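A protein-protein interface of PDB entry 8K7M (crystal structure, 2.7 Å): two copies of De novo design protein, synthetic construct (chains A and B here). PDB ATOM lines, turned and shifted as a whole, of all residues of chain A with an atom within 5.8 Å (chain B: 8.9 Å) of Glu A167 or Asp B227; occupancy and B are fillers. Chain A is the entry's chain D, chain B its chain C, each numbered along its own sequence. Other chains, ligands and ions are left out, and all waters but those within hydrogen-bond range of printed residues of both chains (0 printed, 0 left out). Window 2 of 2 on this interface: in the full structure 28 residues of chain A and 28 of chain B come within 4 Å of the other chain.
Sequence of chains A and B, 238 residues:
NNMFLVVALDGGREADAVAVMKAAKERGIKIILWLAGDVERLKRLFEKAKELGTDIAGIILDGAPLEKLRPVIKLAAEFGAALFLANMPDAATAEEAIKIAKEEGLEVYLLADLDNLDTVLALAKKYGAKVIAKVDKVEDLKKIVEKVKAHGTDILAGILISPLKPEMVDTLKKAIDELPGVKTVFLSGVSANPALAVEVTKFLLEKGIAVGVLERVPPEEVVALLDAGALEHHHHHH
O of Leu B226 lies within hydrogen-bond range of NH2 of Arg B27, 3.2 Å away.
Printed residues of chain A that touch a printed residue of chain B: Pro A166, Glu A167, Val A169 and Asp A170. Hydrophobic or aromatic side chains of chain A that line the printed part of chain B: Pro A166 and Val A169. Among the printed residues, 7 pairs touch across the chains. Among the printed residues, Asp or Glu carboxylates within 4 Å of a Lys or Arg side-chain nitrogen of the other chain: Asp A170 with Arg B27 (3.8 Å).
NE of Arg B27 is in salt-bridge range of OD1 of Asp A170 (3.8 Å).
Among the printed residues, pairs that only touch across the chains: Pro A166 with Leu B225 (3.0 Å), Pro A166 with Ala B224 (3.3 Å), Glu A167 with Asp B227 (3.5 Å), Val A169 with Arg B27 (3.6 Å), Pro A166 with Arg B27 (3.7 Å) and Pro A166 with Asp B227 (3.99 Å).
No position is printed for both chains.
Val A138 touches none of the printed residues of chain B. Of the printed residues of chain B, Pro A166 touches Arg B27 (3.7 Å), Ala B224 (3.3 Å), Leu B225 (3.0 Å) and Asp B227 (3.99 Å). Glu A167 touches one residue of chain B. Of the printed residues of chain B, Val A169 touches Arg B27 (3.6 Å). Printed residues of chain B within 4 Å of Asp A170: Arg B27 (3.8 Å). Val B222 touches none of the printed residues of chain A. Of the printed residues of chain A, Ala B224 touches Pro A166 (3.3 Å). Of the printed residues of chain A, Leu B225 touches Pro A166. Printed residues of chain A within 4 Å of Asp B227: Pro A166 (3.99 Å) and Glu A167 (3.5 Å). The nearest residue of chain B that does not touch Glu A167 is Leu B225 (5.5 Å). The nearest printed residue of chain A that does not touch Asp B227 is Met A168 (5.8 Å).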
ATOM      1  N   VAL A 138       9.461  -6.148 -13.448  1.00  0.00           N
ATOM      2  CA  VAL A 138      10.621  -6.959 -13.062  1.00  0.00           C
ATOM      3  C   VAL A 138      10.926  -8.005 -14.134  1.00  0.00           C
ATOM      4  O   VAL A 138      12.102  -8.251 -14.482  1.00  0.00           O
ATOM      5  CB  VAL A 138      10.368  -7.617 -11.689  1.00  0.00           C
ATOM      6  CG1 VAL A 138      11.486  -8.567 -11.336  1.00  0.00           C
ATOM      7  CG2 VAL A 138      10.244  -6.575 -10.624  1.00  0.00           C
ATOM      8  N   LYS A 165       9.332   0.085  -8.682  1.00  0.00           N
ATOM      9  CA  LYS A 165       8.423  -0.679  -7.848  1.00  0.00           C
ATOM     10  C   LYS A 165       9.212  -1.412  -6.774  1.00  0.00           C
ATOM     11  O   LYS A 165      10.379  -1.736  -6.986  1.00  0.00           O
ATOM     12  CB  LYS A 165       7.664  -1.678  -8.700  1.00  0.00           C
ATOM     13  CG  LYS A 165       6.870  -1.007  -9.789  1.00  0.00           C
ATOM     14  CD  LYS A 165       6.156  -1.985 -10.714  1.00  0.00           C
ATOM     15  CE  LYS A 165       5.350  -1.239 -11.779  1.00  0.00           C
ATOM     16  NZ  LYS A 165       4.554  -2.173 -12.611  1.00  0.00           N
ATOM     17  N   PRO A 166       8.640  -1.648  -5.583  1.00  0.00           N
ATOM     18  CA  PRO A 166       9.417  -2.343  -4.547  1.00  0.00           C
ATOM     19  C   PRO A 166      10.041  -3.642  -5.042  1.00  0.00           C
ATOM     20  O   PRO A 166      11.238  -3.896  -4.806  1.00  0.00           O
ATOM     21  CB  PRO A 166       8.380  -2.563  -3.434  1.00  0.00           C
ATOM     22  CG  PRO A 166       7.047  -2.172  -4.013  1.00  0.00           C
ATOM     23  CD  PRO A 166       7.364  -1.153  -5.045  1.00  0.00           C
ATOM     24  N   GLU A 167       9.272  -4.435  -5.797  1.00  0.00           N
ATOM     25  CA  GLU A 167       9.741  -5.723  -6.294  1.00  0.00           C
ATOM     26  C   GLU A 167      10.873  -5.603  -7.318  1.00  0.00           C
ATOM     27  O   GLU A 167      11.531  -6.607  -7.613  1.00  0.00           O
ATOM     28  CB  GLU A 167       8.564  -6.517  -6.855  1.00  0.00           C
ATOM     29  CG  GLU A 167       7.851  -5.855  -7.986  1.00  0.00           C
ATOM     30  CD  GLU A 167       6.702  -4.993  -7.504  1.00  0.00           C
ATOM     31  OE1 GLU A 167       6.685  -4.645  -6.287  1.00  0.00           O
ATOM     32  OE2 GLU A 167       5.832  -4.658  -8.351  1.00  0.00           O
ATOM     33  N   MET A 168      11.096  -4.418  -7.891  1.00  0.00           N
ATOM     34  CA  MET A 168      12.213  -4.219  -8.801  1.00  0.00           C
ATOM     35  C   MET A 168      13.553  -4.096  -8.092  1.00  0.00           C
ATOM     36  O   MET A 168      14.570  -4.482  -8.681  1.00  0.00           O
ATOM     37  CB  MET A 168      11.997  -2.959  -9.631  1.00  0.00           C
ATOM     38  CG  MET A 168      10.722  -2.968 -10.438  1.00  0.00           C
ATOM     39  SD  MET A 168      10.351  -1.305 -11.089  1.00  0.00           S
ATOM     40  CE  MET A 168       9.668  -1.813 -12.632  1.00  0.00           C
ATOM     41  N   VAL A 169      13.573  -3.653  -6.826  1.00  0.00           N
ATOM     42  CA  VAL A 169      14.830  -3.206  -6.207  1.00  0.00           C
ATOM     43  C   VAL A 169      15.886  -4.313  -6.278  1.00  0.00           C
ATOM     44  O   VAL A 169      16.930  -4.165  -6.929  1.00  0.00           O
ATOM     45  CB  VAL A 169      14.583  -2.735  -4.756  1.00  0.00           C
ATOM     46  CG1 VAL A 169      15.873  -2.356  -4.051  1.00  0.00           C
ATOM     47  CG2 VAL A 169      13.621  -1.560  -4.731  1.00  0.00           C
ATOM     48  N   ASP A 170      15.581  -5.471  -5.687  1.00  0.00           N
ATOM     49  CA  ASP A 170      16.534  -6.574  -5.666  1.00  0.00           C
ATOM     50  C   ASP A 170      16.880  -7.036  -7.074  1.00  0.00           C
ATOM     51  O   ASP A 170      18.060  -7.260  -7.390  1.00  0.00           O
ATOM     52  CB  ASP A 170      15.975  -7.730  -4.844  1.00  0.00           C
ATOM     53  CG  ASP A 170      16.112  -7.484  -3.340  1.00  0.00           C
ATOM     54  OD1 ASP A 170      17.037  -6.724  -2.951  1.00  0.00           O
ATOM     55  OD2 ASP A 170      15.297  -8.027  -2.542  1.00  0.00           O
ATOM     56  N   THR A 171      15.882  -7.137  -7.956  1.00  0.00           N
ATOM     57  CA  THR A 171      16.204  -7.590  -9.300  1.00  0.00           C
ATOM     58  C   THR A 171      17.168  -6.632  -9.971  1.00  0.00           C
ATOM     59  O   THR A 171      18.182  -7.063 -10.544  1.00  0.00           O
ATOM     60  CB  THR A 171      14.939  -7.772 -10.116  1.00  0.00           C
ATOM     61  OG1 THR A 171      14.190  -8.866  -9.565  1.00  0.00           O
ATOM     62  CG2 THR A 171      15.282  -8.033 -11.554  1.00  0.00           C
ATOM     63  N   ALA B  19       9.174 -10.370   9.098  1.00  0.00           N
ATOM     64  CA  ALA B  19       9.457 -10.292   7.669  1.00  0.00           C
ATOM     65  C   ALA B  19      10.258  -9.037   7.352  1.00  0.00           C
ATOM     66  O   ALA B  19      11.163  -9.059   6.510  1.00  0.00           O
ATOM     67  CB  ALA B  19       8.149 -10.321   6.880  1.00  0.00           C
ATOM     68  N   VAL B  20       9.938  -7.939   8.038  1.00  0.00           N
ATOM     69  CA  VAL B  20      10.694  -6.696   7.899  1.00  0.00           C
ATOM     70  C   VAL B  20      12.141  -6.887   8.341  1.00  0.00           C
ATOM     71  O   VAL B  20      13.081  -6.453   7.659  1.00  0.00           O
ATOM     72  CB  VAL B  20      10.003  -5.566   8.683  1.00  0.00           C
ATOM     73  CG1 VAL B  20      10.932  -4.382   8.854  1.00  0.00           C
ATOM     74  CG2 VAL B  20       8.734  -5.143   7.972  1.00  0.00           C
ATOM     75  N   ALA B  23      13.973  -9.051   5.794  1.00  0.00           N
ATOM     76  CA  ALA B  23      14.268  -8.345   4.555  1.00  0.00           C
ATOM     77  C   ALA B  23      15.384  -7.327   4.752  1.00  0.00           C
ATOM     78  O   ALA B  23      16.253  -7.168   3.885  1.00  0.00           O
ATOM     79  CB  ALA B  23      12.999  -7.679   4.019  1.00  0.00           C
ATOM     80  N   GLU B  26      18.722  -9.080   4.945  1.00  0.00           N
ATOM     81  CA  GLU B  26      19.119  -9.456   3.600  1.00  0.00           C
ATOM     82  C   GLU B  26      19.582  -8.274   2.766  1.00  0.00           C
ATOM     83  O   GLU B  26      20.481  -8.432   1.934  1.00  0.00           O
ATOM     84  CB  GLU B  26      17.994 -10.198   2.916  1.00  0.00           C
ATOM     85  CG  GLU B  26      17.771 -11.507   3.627  1.00  0.00           C
ATOM     86  CD  GLU B  26      16.488 -12.151   3.238  1.00  0.00           C
ATOM     87  OE1 GLU B  26      15.792 -11.580   2.352  1.00  0.00           O
ATOM     88  OE2 GLU B  26      16.194 -13.229   3.812  1.00  0.00           O
ATOM     89  N   ARG B  27      19.005  -7.092   2.945  1.00  0.00           N
ATOM     90  CA  ARG B  27      19.395  -5.993   2.074  1.00  0.00           C
ATOM     91  C   ARG B  27      20.495  -5.118   2.682  1.00  0.00           C
ATOM     92  O   ARG B  27      20.899  -4.131   2.062  1.00  0.00           O
ATOM     93  CB  ARG B  27      18.188  -5.121   1.712  1.00  0.00           C
ATOM     94  CG  ARG B  27      17.199  -5.692   0.705  1.00  0.00           C
ATOM     95  CD  ARG B  27      16.083  -4.688   0.580  1.00  0.00           C
ATOM     96  NE  ARG B  27      14.983  -5.000  -0.327  1.00  0.00           N
ATOM     97  CZ  ARG B  27      14.254  -4.064  -0.929  1.00  0.00           C
ATOM     98  NH1 ARG B  27      14.518  -2.776  -0.772  1.00  0.00           N
ATOM     99  NH2 ARG B  27      13.206  -4.422  -1.668  1.00  0.00           N
ATOM    100  N   PRO B 219       3.797  -2.139  10.056  1.00  0.00           N
ATOM    101  CA  PRO B 219       4.763  -3.070   9.442  1.00  0.00           C
ATOM    102  C   PRO B 219       4.270  -3.709   8.165  1.00  0.00           C
ATOM    103  O   PRO B 219       5.084  -4.139   7.349  1.00  0.00           O
ATOM    104  CB  PRO B 219       4.981  -4.121  10.540  1.00  0.00           C
ATOM    105  CG  PRO B 219       4.645  -3.413  11.805  1.00  0.00           C
ATOM    106  CD  PRO B 219       3.527  -2.467  11.462  1.00  0.00           C
ATOM    107  N   GLU B 220       2.961  -3.832   7.990  1.00  0.00           N
ATOM    108  CA  GLU B 220       2.432  -4.370   6.749  1.00  0.00           C
ATOM    109  C   GLU B 220       2.824  -3.495   5.554  1.00  0.00           C
ATOM    110  O   GLU B 220       3.115  -4.009   4.463  1.00  0.00           O
ATOM    111  CB  GLU B 220       0.930  -4.500   6.909  1.00  0.00           C
ATOM    112  CG  GLU B 220       0.225  -5.285   5.891  1.00  0.00           C
ATOM    113  CD  GLU B 220      -1.260  -5.332   6.175  1.00  0.00           C
ATOM    114  OE1 GLU B 220      -1.755  -4.516   6.999  1.00  0.00           O
ATOM    115  OE2 GLU B 220      -1.930  -6.232   5.622  1.00  0.00           O
ATOM    116  N   GLU B 221       2.844  -2.164   5.747  1.00  0.00           N
ATOM    117  CA  GLU B 221       3.261  -1.237   4.693  1.00  0.00           C
ATOM    118  C   GLU B 221       4.747  -1.353   4.396  1.00  0.00           C
ATOM    119  O   GLU B 221       5.181  -1.184   3.248  1.00  0.00           O
ATOM    120  CB  GLU B 221       2.937   0.208   5.079  1.00  0.00           C
ATOM    121  CG  GLU B 221       1.483   0.487   5.257  1.00  0.00           C
ATOM    122  CD  GLU B 221       0.687   0.001   4.075  1.00  0.00           C
ATOM    123  OE1 GLU B 221       1.146   0.206   2.937  1.00  0.00           O
ATOM    124  OE2 GLU B 221      -0.390  -0.604   4.276  1.00  0.00           O
ATOM    125  N   VAL B 222       5.552  -1.557   5.429  1.00  0.00           N
ATOM    126  CA  VAL B 222       6.973  -1.735   5.213  1.00  0.00           C
ATOM    127  C   VAL B 222       7.223  -3.077   4.531  1.00  0.00           C
ATOM    128  O   VAL B 222       8.111  -3.203   3.682  1.00  0.00           O
ATOM    129  CB  VAL B 222       7.711  -1.610   6.554  1.00  0.00           C
ATOM    130  CG1 VAL B 222       9.207  -1.692   6.369  1.00  0.00           C
ATOM    131  CG2 VAL B 222       7.332  -0.321   7.201  1.00  0.00           C
ATOM    132  N   VAL B 223       6.427  -4.091   4.867  1.00  0.00           N
ATOM    133  CA  VAL B 223       6.554  -5.370   4.192  1.00  0.00           C
ATOM    134  C   VAL B 223       6.290  -5.203   2.718  1.00  0.00           C
ATOM    135  O   VAL B 223       7.017  -5.747   1.884  1.00  0.00           O
ATOM    136  CB  VAL B 223       5.614  -6.419   4.807  1.00  0.00           C
ATOM    137  CG1 VAL B 223       5.384  -7.553   3.801  1.00  0.00           C
ATOM    138  CG2 VAL B 223       6.227  -6.962   6.068  1.00  0.00           C
ATOM    139  N   ALA B 224       5.274  -4.413   2.368  1.00  0.00           N
ATOM    140  CA  ALA B 224       5.049  -4.137   0.945  1.00  0.00           C
ATOM    141  C   ALA B 224       6.214  -3.357   0.330  1.00  0.00           C
ATOM    142  O   ALA B 224       6.642  -3.649  -0.794  1.00  0.00           O
ATOM    143  CB  ALA B 224       3.732  -3.403   0.746  1.00  0.00           C
ATOM    144  N   LEU B 225       6.744  -2.366   1.057  1.00  0.00           N
ATOM    145  CA  LEU B 225       7.831  -1.547   0.528  1.00  0.00           C
ATOM    146  C   LEU B 225       9.080  -2.376   0.220  1.00  0.00           C
ATOM    147  O   LEU B 225       9.769  -2.136  -0.778  1.00  0.00           O
ATOM    148  CB  LEU B 225       8.172  -0.451   1.519  1.00  0.00           C
ATOM    149  CG  LEU B 225       9.351   0.427   1.127  1.00  0.00           C
ATOM    150  CD1 LEU B 225       8.937   1.422   0.060  1.00  0.00           C
ATOM    151  CD2 LEU B 225       9.881   1.097   2.363  1.00  0.00           C
ATOM    152  N   LEU B 226       9.429  -3.311   1.091  1.00  0.00           N
ATOM    153  CA  LEU B 226      10.575  -4.164   0.840  1.00  0.00           C
ATOM    154  C   LEU B 226      10.222  -5.407   0.066  1.00  0.00           C
ATOM    155  O   LEU B 226      11.081  -6.279  -0.081  1.00  0.00           O
ATOM    156  CB  LEU B 226      11.254  -4.577   2.138  1.00  0.00           C
ATOM    157  CG  LEU B 226      11.601  -3.425   3.060  1.00  0.00           C
ATOM    158  CD1 LEU B 226      12.135  -4.018   4.346  1.00  0.00           C
ATOM    159  CD2 LEU B 226      12.621  -2.522   2.384  1.00  0.00           C
ATOM    160  N   ASP B 227       9.003  -5.506  -0.455  1.00  0.00           N
ATOM    161  CA  ASP B 227       8.587  -6.695  -1.199  1.00  0.00           C
ATOM    162  C   ASP B 227       8.967  -7.964  -0.434  1.00  0.00           C
ATOM    163  O   ASP B 227       9.731  -8.805  -0.910  1.00  0.00           O
ATOM    164  CB  ASP B 227       9.198  -6.684  -2.604  1.00  0.00           C
ATOM    165  CG  ASP B 227       8.580  -7.721  -3.515  1.00  0.00           C
ATOM    166  OD1 ASP B 227       7.328  -7.764  -3.595  1.00  0.00           O
ATOM    167  OD2 ASP B 227       9.352  -8.496  -4.137  1.00  0.00           O
ATOM    168  N   ALA B 228       8.511  -8.043   0.812  1.00  0.00           N
ATOM    169  CA  ALA B 228       8.945  -9.077   1.737  1.00  0.00           C
ATOM    170  C   ALA B 228       7.820 -10.035   2.097  1.00  0.00           C
ATOM    171  O   ALA B 228       7.831 -10.627   3.175  1.00  0.00           O
ATOM    172  CB  ALA B 228       9.545  -8.450   2.995  1.00  0.00           C
ATOM    173  N   GLY B 229       6.859 -10.232   1.201  1.00  0.00           N
ATOM    174  CA  GLY B 229       5.824 -11.211   1.475  1.00  0.00           C
ATOM    175  C   GLY B 229       6.330 -12.642   1.501  1.00  0.00           C
ATOM    176  O   GLY B 229       5.796 -13.475   2.243  1.00  0.00           O
ATOM    177  N   ALA B 230       7.381 -12.946   0.737  1.00  0.00           N
ATOM    178  CA  ALA B 230       7.928 -14.306   0.669  1.00  0.00           C
ATOM    179  C   ALA B 230       8.489 -14.810   2.011  1.00  0.00           C
ATOM    180  O   ALA B 230       9.012 -14.041   2.830  1.00  0.00           O
ATOM    181  CB  ALA B 230       9.013 -14.377  -0.421  1.00  0.00           C
